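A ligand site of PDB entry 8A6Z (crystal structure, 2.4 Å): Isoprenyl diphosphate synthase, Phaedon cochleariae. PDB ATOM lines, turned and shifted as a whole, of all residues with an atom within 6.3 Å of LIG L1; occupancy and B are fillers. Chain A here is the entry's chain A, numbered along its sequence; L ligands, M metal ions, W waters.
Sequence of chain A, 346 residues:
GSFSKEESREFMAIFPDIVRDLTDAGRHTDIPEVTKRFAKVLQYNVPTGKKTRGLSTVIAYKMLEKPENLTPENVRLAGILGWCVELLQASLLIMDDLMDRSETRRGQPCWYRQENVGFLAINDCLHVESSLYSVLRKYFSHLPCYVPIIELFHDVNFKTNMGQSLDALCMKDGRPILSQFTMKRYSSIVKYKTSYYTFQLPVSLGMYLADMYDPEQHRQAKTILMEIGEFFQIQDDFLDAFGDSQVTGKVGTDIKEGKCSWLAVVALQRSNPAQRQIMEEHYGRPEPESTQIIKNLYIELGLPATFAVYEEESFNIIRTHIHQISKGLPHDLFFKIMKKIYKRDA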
ATOM      1  N   THR A  48       1.451  14.057 -21.578  1.00  0.00           N
ATOM      2  CA  THR A  48       0.661  15.196 -22.136  1.00  0.00           C
ATOM      3  C   THR A  48       1.578  16.361 -22.570  1.00  0.00           C
ATOM      4  O   THR A  48       1.033  17.341 -23.114  1.00  0.00           O
ATOM      5  CB  THR A  48      -0.442  15.647 -21.159  1.00  0.00           C
ATOM      6  OG1 THR A  48       0.145  16.222 -19.989  1.00  0.00           O
ATOM      7  CG2 THR A  48      -1.354  14.507 -20.760  1.00  0.00           C
ATOM      8  N   GLY A  49       2.898  16.262 -22.353  1.00  0.00           N
ATOM      9  CA  GLY A  49       3.878  17.286 -22.762  1.00  0.00           C
ATOM     10  C   GLY A  49       4.229  17.175 -24.236  1.00  0.00           C
ATOM     11  O   GLY A  49       3.648  16.322 -24.914  1.00  0.00           O
ATOM     12  N   LYS A  50       5.180  17.999 -24.703  1.00  0.00           N
ATOM     13  CA  LYS A  50       5.657  18.029 -26.115  1.00  0.00           C
ATOM     14  C   LYS A  50       6.506  16.783 -26.427  1.00  0.00           C
ATOM     15  O   LYS A  50       6.645  16.462 -27.625  1.00  0.00           O
ATOM     16  CB  LYS A  50       6.477  19.291 -26.396  1.00  0.00           C
ATOM     17  CG  LYS A  50       5.695  20.599 -26.347  1.00  0.00           C
ATOM     18  CD  LYS A  50       6.531  21.809 -26.701  1.00  0.00           C
ATOM     19  CE  LYS A  50       7.769  21.989 -25.851  1.00  0.00           C
ATOM     20  NZ  LYS A  50       7.461  21.936 -24.404  1.00  0.00           N
ATOM     21  N   LYS A  51       7.096  16.170 -25.401  1.00  0.00           N
ATOM     22  CA  LYS A  51       7.836  14.881 -25.478  1.00  0.00           C
ATOM     23  C   LYS A  51       9.125  15.027 -26.293  1.00  0.00           C
ATOM     24  O   LYS A  51       9.570  14.010 -26.878  1.00  0.00           O
ATOM     25  CB  LYS A  51       6.902  13.785 -26.022  1.00  0.00           C
ATOM     26  CG  LYS A  51       5.751  13.424 -25.100  1.00  0.00           C
ATOM     27  CD  LYS A  51       4.820  12.361 -25.653  1.00  0.00           C
ATOM     28  CE  LYS A  51       3.885  12.888 -26.719  1.00  0.00           C
ATOM     29  NZ  LYS A  51       2.932  13.895 -26.179  1.00  0.00           N
ATOM     30  N   THR A  52       9.739  16.216 -26.312  1.00  0.00           N
ATOM     31  CA  THR A  52      10.951  16.521 -27.114  1.00  0.00           C
ATOM     32  C   THR A  52      12.127  15.684 -26.602  1.00  0.00           C
ATOM     33  O   THR A  52      12.845  15.116 -27.458  1.00  0.00           O
ATOM     34  CB  THR A  52      11.272  18.019 -27.094  1.00  0.00           C
ATOM     35  OG1 THR A  52      10.163  18.685 -27.691  1.00  0.00           O
ATOM     36  CG2 THR A  52      12.537  18.378 -27.836  1.00  0.00           C
ATOM     37  N   ARG A  53      12.326  15.612 -25.279  1.00  0.00           N
ATOM     38  CA  ARG A  53      13.433  14.832 -24.667  1.00  0.00           C
ATOM     39  C   ARG A  53      13.339  13.386 -25.170  1.00  0.00           C
ATOM     40  O   ARG A  53      14.337  12.893 -25.751  1.00  0.00           O
ATOM     41  CB  ARG A  53      13.369  14.901 -23.135  1.00  0.00           C
ATOM     42  CG  ARG A  53      13.618  16.285 -22.545  1.00  0.00           C
ATOM     43  CD  ARG A  53      13.203  16.395 -21.087  1.00  0.00           C
ATOM     44  NE  ARG A  53      13.222  17.768 -20.582  1.00  0.00           N
ATOM     45  CZ  ARG A  53      12.307  18.698 -20.840  1.00  0.00           C
ATOM     46  NH1 ARG A  53      11.262  18.418 -21.613  1.00  0.00           N
ATOM     47  NH2 ARG A  53      12.437  19.918 -20.334  1.00  0.00           N
ATOM     48  N   GLU A  86      11.190  10.851 -20.038  1.00  0.00           N
ATOM     49  CA  GLU A  86       9.881  11.517 -19.822  1.00  0.00           C
ATOM     50  C   GLU A  86       9.376  11.191 -18.411  1.00  0.00           C
ATOM     51  O   GLU A  86       8.743  12.094 -17.788  1.00  0.00           O
ATOM     52  CB  GLU A  86       8.862  11.099 -20.894  1.00  0.00           C
ATOM     53  CG  GLU A  86       9.168  11.649 -22.276  1.00  0.00           C
ATOM     54  CD  GLU A  86       9.287  13.157 -22.382  1.00  0.00           C
ATOM     55  OE1 GLU A  86       8.634  13.864 -21.583  1.00  0.00           O
ATOM     56  OE2 GLU A  86      10.035  13.629 -23.274  1.00  0.00           O
ATOM     57  N   GLN A  89      11.272  13.594 -16.346  1.00  0.00           N
ATOM     58  CA  GLN A  89      10.660  14.929 -16.592  1.00  0.00           C
ATOM     59  C   GLN A  89       9.378  15.035 -15.756  1.00  0.00           C
ATOM     60  O   GLN A  89       9.211  16.044 -15.050  1.00  0.00           O
ATOM     61  CB  GLN A  89      10.379  15.168 -18.072  1.00  0.00           C
ATOM     62  CG  GLN A  89       9.510  16.398 -18.364  1.00  0.00           C
ATOM     63  CD  GLN A  89      10.166  17.737 -18.107  1.00  0.00           C
ATOM     64  OE1 GLN A  89      10.983  17.890 -17.204  1.00  0.00           O
ATOM     65  NE2 GLN A  89       9.779  18.729 -18.890  1.00  0.00           N
ATOM     66  N   LEU A  93       8.543  17.824 -12.751  1.00  0.00           N
ATOM     67  CA  LEU A  93       7.439  18.805 -12.985  1.00  0.00           C
ATOM     68  C   LEU A  93       6.427  18.753 -11.826  1.00  0.00           C
ATOM     69  O   LEU A  93       5.882  19.823 -11.472  1.00  0.00           O
ATOM     70  CB  LEU A  93       6.762  18.495 -14.324  1.00  0.00           C
ATOM     71  CG  LEU A  93       7.220  19.350 -15.503  1.00  0.00           C
ATOM     72  CD1 LEU A  93       8.740  19.402 -15.590  1.00  0.00           C
ATOM     73  CD2 LEU A  93       6.622  18.855 -16.812  1.00  0.00           C
ATOM     74  N   ARG A 105      -0.452  23.087 -15.284  1.00  0.00           N
ATOM     75  CA  ARG A 105       0.624  22.377 -16.017  1.00  0.00           C
ATOM     76  C   ARG A 105       0.007  21.678 -17.227  1.00  0.00           C
ATOM     77  O   ARG A 105      -0.990  20.959 -17.032  1.00  0.00           O
ATOM     78  CB  ARG A 105       1.322  21.373 -15.087  1.00  0.00           C
ATOM     79  CG  ARG A 105       2.327  20.464 -15.784  1.00  0.00           C
ATOM     80  CD  ARG A 105       3.511  21.223 -16.372  1.00  0.00           C
ATOM     81  NE  ARG A 105       4.433  21.689 -15.345  1.00  0.00           N
ATOM     82  CZ  ARG A 105       5.509  22.446 -15.577  1.00  0.00           C
ATOM     83  NH1 ARG A 105       5.804  22.824 -16.810  1.00  0.00           N
ATOM     84  NH2 ARG A 105       6.284  22.804 -14.577  1.00  0.00           N
ATOM     85  N   ARG A 106       0.544  21.927 -18.426  1.00  0.00           N
ATOM     86  CA  ARG A 106       0.144  21.271 -19.699  1.00  0.00           C
ATOM     87  C   ARG A 106      -1.371  21.405 -19.918  1.00  0.00           C
ATOM     88  O   ARG A 106      -1.974  20.445 -20.451  1.00  0.00           O
ATOM     89  CB  ARG A 106       0.580  19.804 -19.702  1.00  0.00           C
ATOM     90  CG  ARG A 106       2.091  19.612 -19.731  1.00  0.00           C
ATOM     91  CD  ARG A 106       2.460  18.186 -19.389  1.00  0.00           C
ATOM     92  NE  ARG A 106       3.889  17.948 -19.467  1.00  0.00           N
ATOM     93  CZ  ARG A 106       4.503  16.850 -19.036  1.00  0.00           C
ATOM     94  NH1 ARG A 106       3.820  15.858 -18.486  1.00  0.00           N
ATOM     95  NH2 ARG A 106       5.816  16.746 -19.153  1.00  0.00           N
ATOM     96  N   LYS A 193      20.215  22.772 -13.554  1.00  0.00           N
ATOM     97  CA  LYS A 193      18.726  22.687 -13.472  1.00  0.00           C
ATOM     98  C   LYS A 193      18.147  22.026 -14.728  1.00  0.00           C
ATOM     99  O   LYS A 193      17.256  21.159 -14.578  1.00  0.00           O
ATOM    100  CB  LYS A 193      18.150  24.091 -13.303  1.00  0.00           C
ATOM    101  CG  LYS A 193      16.642  24.149 -13.128  1.00  0.00           C
ATOM    102  CD  LYS A 193      16.130  25.504 -12.702  1.00  0.00           C
ATOM    103  CE  LYS A 193      15.430  26.278 -13.790  1.00  0.00           C
ATOM    104  NZ  LYS A 193      14.387  27.166 -13.221  1.00  0.00           N
ATOM    105  N   THR A 194      18.603  22.422 -15.925  1.00  0.00           N
ATOM    106  CA  THR A 194      17.923  22.137 -17.219  1.00  0.00           C
ATOM    107  C   THR A 194      18.805  21.284 -18.140  1.00  0.00           C
ATOM    108  O   THR A 194      18.349  20.196 -18.531  1.00  0.00           O
ATOM    109  CB  THR A 194      17.516  23.440 -17.911  1.00  0.00           C
ATOM    110  OG1 THR A 194      16.520  24.090 -17.122  1.00  0.00           O
ATOM    111  CG2 THR A 194      16.971  23.225 -19.314  1.00  0.00           C
ATOM    112  N   TYR A 197      19.739  17.141 -17.974  1.00  0.00           N
ATOM    113  CA  TYR A 197      18.629  16.157 -18.115  1.00  0.00           C
ATOM    114  C   TYR A 197      17.871  16.393 -19.434  1.00  0.00           C
ATOM    115  O   TYR A 197      17.411  15.399 -20.041  1.00  0.00           O
ATOM    116  CB  TYR A 197      17.723  16.154 -16.885  1.00  0.00           C
ATOM    117  CG  TYR A 197      16.476  17.008 -16.965  1.00  0.00           C
ATOM    118  CD1 TYR A 197      15.257  16.466 -17.338  1.00  0.00           C
ATOM    119  CD2 TYR A 197      16.506  18.351 -16.650  1.00  0.00           C
ATOM    120  CE1 TYR A 197      14.105  17.229 -17.405  1.00  0.00           C
ATOM    121  CE2 TYR A 197      15.368  19.143 -16.710  1.00  0.00           C
ATOM    122  CZ  TYR A 197      14.163  18.577 -17.097  1.00  0.00           C
ATOM    123  OH  TYR A 197      13.038  19.358 -17.169  1.00  0.00           O
ATOM    124  N   THR A 198      17.739  17.634 -19.888  1.00  0.00           N
ATOM    125  CA  THR A 198      16.888  17.990 -21.052  1.00  0.00           C
ATOM    126  C   THR A 198      17.620  17.661 -22.360  1.00  0.00           C
ATOM    127  O   THR A 198      16.955  17.146 -23.284  1.00  0.00           O
ATOM    128  CB  THR A 198      16.424  19.444 -20.980  1.00  0.00           C
ATOM    129  OG1 THR A 198      15.639  19.526 -19.784  1.00  0.00           O
ATOM    130  CG2 THR A 198      15.597  19.871 -22.184  1.00  0.00           C
ATOM    131  N   PHE A 232      17.592  27.278 -24.574  1.00  0.00           N
ATOM    132  CA  PHE A 232      16.246  26.708 -24.306  1.00  0.00           C
ATOM    133  C   PHE A 232      15.627  27.359 -23.065  1.00  0.00           C
ATOM    134  O   PHE A 232      14.413  27.675 -23.103  1.00  0.00           O
ATOM    135  CB  PHE A 232      16.313  25.182 -24.152  1.00  0.00           C
ATOM    136  CG  PHE A 232      15.004  24.506 -23.832  1.00  0.00           C
ATOM    137  CD1 PHE A 232      14.091  24.206 -24.845  1.00  0.00           C
ATOM    138  CD2 PHE A 232      14.676  24.166 -22.529  1.00  0.00           C
ATOM    139  CE1 PHE A 232      12.889  23.577 -24.556  1.00  0.00           C
ATOM    140  CE2 PHE A 232      13.473  23.536 -22.241  1.00  0.00           C
ATOM    141  CZ  PHE A 232      12.576  23.251 -23.249  1.00  0.00           C
ATOM    142  N   GLN A 233      16.400  27.524 -21.978  1.00  0.00           N
ATOM    143  CA  GLN A 233      15.854  27.988 -20.678  1.00  0.00           C
ATOM    144  C   GLN A 233      15.551  29.484 -20.766  1.00  0.00           C
ATOM    145  O   GLN A 233      14.557  29.913 -20.138  1.00  0.00           O
ATOM    146  CB  GLN A 233      16.800  27.733 -19.501  1.00  0.00           C
ATOM    147  CG  GLN A 233      16.145  27.967 -18.143  1.00  0.00           C
ATOM    148  CD  GLN A 233      14.871  27.166 -17.950  1.00  0.00           C
ATOM    149  OE1 GLN A 233      14.835  25.965 -18.194  1.00  0.00           O
ATOM    150  NE2 GLN A 233      13.813  27.839 -17.514  1.00  0.00           N
ATOM    151  N   ASP A 236      12.309  29.708 -22.100  1.00  0.00           N
ATOM    152  CA  ASP A 236      11.287  29.317 -21.078  1.00  0.00           C
ATOM    153  C   ASP A 236      10.996  30.530 -20.189  1.00  0.00           C
ATOM    154  O   ASP A 236       9.811  30.813 -19.953  1.00  0.00           O
ATOM    155  CB  ASP A 236      11.727  28.091 -20.281  1.00  0.00           C
ATOM    156  CG  ASP A 236      10.639  27.529 -19.384  1.00  0.00           C
ATOM    157  OD1 ASP A 236       9.742  26.830 -19.886  1.00  0.00           O
ATOM    158  OD2 ASP A 236      10.695  27.806 -18.174  1.00  0.00           O
ATOM    159  N   LYS A 250       0.671  26.765 -19.115  1.00  0.00           N
ATOM    160  CA  LYS A 250       1.007  27.122 -17.705  1.00  0.00           C
ATOM    161  C   LYS A 250       0.942  28.636 -17.512  1.00  0.00           C
ATOM    162  O   LYS A 250       1.262  29.381 -18.461  1.00  0.00           O
ATOM    163  CB  LYS A 250       2.397  26.589 -17.325  1.00  0.00           C
ATOM    164  CG  LYS A 250       3.572  27.253 -18.026  1.00  0.00           C
ATOM    165  CD  LYS A 250       4.704  26.299 -18.348  1.00  0.00           C
ATOM    166  CE  LYS A 250       5.829  26.954 -19.115  1.00  0.00           C
ATOM    167  NZ  LYS A 250       7.010  26.074 -19.206  1.00  0.00           N
ATOM    168  N   ARG A 344       9.934  28.978 -30.927  1.00  0.00           N
ATOM    169  CA  ARG A 344       8.787  28.264 -30.306  1.00  0.00           C
ATOM    170  C   ARG A 344       7.975  29.280 -29.478  1.00  0.00           C
ATOM    171  O   ARG A 344       8.551  30.302 -29.051  1.00  0.00           O
ATOM    172  CB  ARG A 344       9.271  27.069 -29.472  1.00  0.00           C
ATOM    173  CG  ARG A 344       9.969  27.409 -28.155  1.00  0.00           C
ATOM    174  CD  ARG A 344      10.660  26.194 -27.566  1.00  0.00           C
ATOM    175  NE  ARG A 344      11.366  26.455 -26.308  1.00  0.00           N
ATOM    176  CZ  ARG A 344      10.831  26.377 -25.089  1.00  0.00           C
ATOM    177  NH1 ARG A 344       9.558  26.047 -24.927  1.00  0.00           N
ATOM    178  NH2 ARG A 344      11.567  26.641 -24.029  1.00  0.00           N
ATOM    179  N   ALA A 346       5.576  27.655 -27.308  1.00  0.00           N
ATOM    180  CA  ALA A 346       5.228  26.676 -26.260  1.00  0.00           C
ATOM    181  C   ALA A 346       6.470  25.844 -25.908  1.00  0.00           C
ATOM    182  O   ALA A 346       6.453  25.015 -24.983  1.00  0.00           O
ATOM    183  CB  ALA A 346       4.085  25.793 -26.707  1.00  0.00           C
ATOM    184  OXT ALA A 346       7.496  25.989 -26.556  1.00  0.00           O
HETATM  185  C1  LIG L   1       9.548  22.204 -18.942  1.00  0.00           C
HETATM  186  O1  LIG L   1      10.069  21.545 -20.124  1.00  0.00           O
HETATM  187  C2  LIG L   1      10.606  22.366 -17.887  1.00  0.00           C
HETATM  188  C3  LIG L   1      11.834  23.124 -18.319  1.00  0.00           C
HETATM  189  C4  LIG L   1      13.043  22.591 -18.297  1.00  0.00           C
HETATM  190  C5  LIG L   1      11.595  24.526 -18.775  1.00  0.00           C
HETATM  191  P1  LIG L   1       9.159  21.523 -21.460  1.00  0.00           P
HETATM  192  O2  LIG L   1       9.878  20.769 -22.531  1.00  0.00           O
HETATM  193  O3  LIG L   1       8.733  22.927 -21.740  1.00  0.00           O
HETATM  194  O4  LIG L   1       7.861  20.701 -20.977  1.00  0.00           O
HETATM  195  P2  LIG L   1       6.831  19.568 -21.522  1.00  0.00           P
HETATM  196  O5  LIG L   1       6.527  19.877 -22.970  1.00  0.00           O
HETATM  197  O6  LIG L   1       7.514  18.240 -21.363  1.00  0.00           O
HETATM  198  O7  LIG L   1       5.617  19.691 -20.644  1.00  0.00           O
HETATM  199  C1  LG2 L   2      13.175  24.411 -14.817  1.00  0.00           C
HETATM  200  O1  LG2 L   2      12.055  24.664 -13.956  1.00  0.00           O
HETATM  201  C2  LG2 L   2      13.355  22.926 -15.139  1.00  0.00           C
HETATM  202  C3  LG2 L   2      12.870  21.868 -14.169  1.00  0.00           C
HETATM  203  C4  LG2 L   2      13.675  21.264 -13.299  1.00  0.00           C
HETATM  204  C5  LG2 L   2      11.442  21.495 -14.279  1.00  0.00           C
HETATM  205  P1  LG2 L   2      11.094  25.870 -14.186  1.00  0.00           P
HETATM  206  O2  LG2 L   2      10.272  26.045 -12.994  1.00  0.00           O
HETATM  207  O3  LG2 L   2      11.749  27.052 -14.715  1.00  0.00           O
HETATM  208  O4  LG2 L   2      10.089  25.201 -15.170  1.00  0.00           O
HETATM  209  P2  LG2 L   2       8.607  25.608 -15.658  1.00  0.00           P
HETATM  210  O5  LG2 L   2       8.704  27.013 -16.184  1.00  0.00           O
HETATM  211  O6  LG2 L   2       8.233  24.614 -16.730  1.00  0.00           O
HETATM  212  O7  LG2 L   2       7.727  25.500 -14.444  1.00  0.00           O
HETATM  213 MN    MN M   1      10.071  28.569 -16.342  1.00  0.00          MN
HETATM  214  O   HOH W   1       9.783  25.227 -21.954  1.00  0.00           O
HETATM  215  O   HOH W   2       7.087  16.033 -22.669  1.00  0.00           O
HETATM  216  O   HOH W   3       9.197  18.142 -23.938  1.00  0.00           O
HETATM  217  O   HOH W   4       6.424  24.070 -20.718  1.00  0.00           O
HETATM  218  O   HOH W   5      10.790  20.526 -25.035  1.00  0.00           O
HETATM  219  O   HOH W   6       5.152  22.071 -19.590  1.00  0.00           O
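Gly 49 touches LIG L1 (CA to O7, 3.6 Å).
OG1 of Thr 194 touches C4 of LIG L1 (3.96 Å).
Tyr 197 touches LIG L1.
Phe 232 touches LIG L1.
Gln 233 touches LIG L1.
Asp 236 touches LIG L1.
Hydrophobic or aromatic side chains that line LIG L1: Phe 232.
Of the 21 residues printed, 10 come within 4 Å of LIG L1.
The chain-end carboxylate (O) of Ala 346 is in salt-bridge range of the side-chain amino group (NZ) of Lys 50, 3.3 Å away.
The side-chain amide nitrogen of Gln 89 lies close to the guanidinium group of Arg 53, 3.1 Å away.
NH2 of Arg 53 lies within hydrogen-bond range of OH of Tyr 197 (3.3 Å).
NE of Arg 53 sits at hydrogen-bond distance from OG1 of Thr 198, at 3.1 Å.
The side-chain carboxylate (OD1) of Asp 236 is in salt-bridge range of the side-chain amino group (NZ) of Lys 250 (2.9 Å).
The side-chain hydroxyl of Thr 194 lies within hydrogen-bond range of the side-chain amide oxygen of Gln 233.
NH2 of Arg 344 sits at hydrogen-bond distance from O of Phe 232 (3.2 Å).
The side-chain hydroxyl (OG1) of Thr 198 is in hydrogen-bond range of the backbone carbonyl oxygen (O) of Thr 194, 3.1 Å away.
Water W1 lies within hydrogen-bond range of an oxygen (O3) of LIG L1, the side-chain carboxylate (OD1) of Asp 236 and the guanidinium group (NH2) of Arg 344.
Water W2 lies within hydrogen-bond range of O6 of LIG L1, N of Lys 51, OE1 of Glu 86 and N of Lys 50.
Water W6 lies within hydrogen-bond range of O7 of LIG L1 (2.6 Å) and NH1 of Arg 105 (3.0 Å).
Water W5 lies within hydrogen-bond range of an oxygen (O2) of LIG L1 (2.7 Å) and the side-chain hydroxyl of Thr 52 (3.3 Å).
Water W4 bridges NZ of Lys 250 (2.6 Å) and O3 of LIG L1 (2.8 Å).
N of Lys 50 is in hydrogen-bond range of O5 of LIG L1.
The side-chain amino group of Lys 50 is in salt-bridge range of an oxygen (O5) of LIG L1 (2.7 Å).
The guanidinium group (NE) of Arg 106 lies within salt-bridge range of an oxygen (O7) of LIG L1, 2.7 Å away.
NH1 of Arg 53 is in salt-bridge range of O2 of LIG L1, 2.9 Å away.
NE2 of Gln 89 sits at hydrogen-bond distance from O1 of LIG L1 (3.1 Å).
NH1 of Arg 105 lies within salt-bridge range of O6 of LG2 L2, at 3.0 Å.
An oxygen (O6) of LG2 L2 is in salt-bridge range of the side-chain amino group (NZ) of Lys 250, at 3.1 Å.
O3 of LG2 L2 is in salt-bridge range of NZ of Lys 193.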
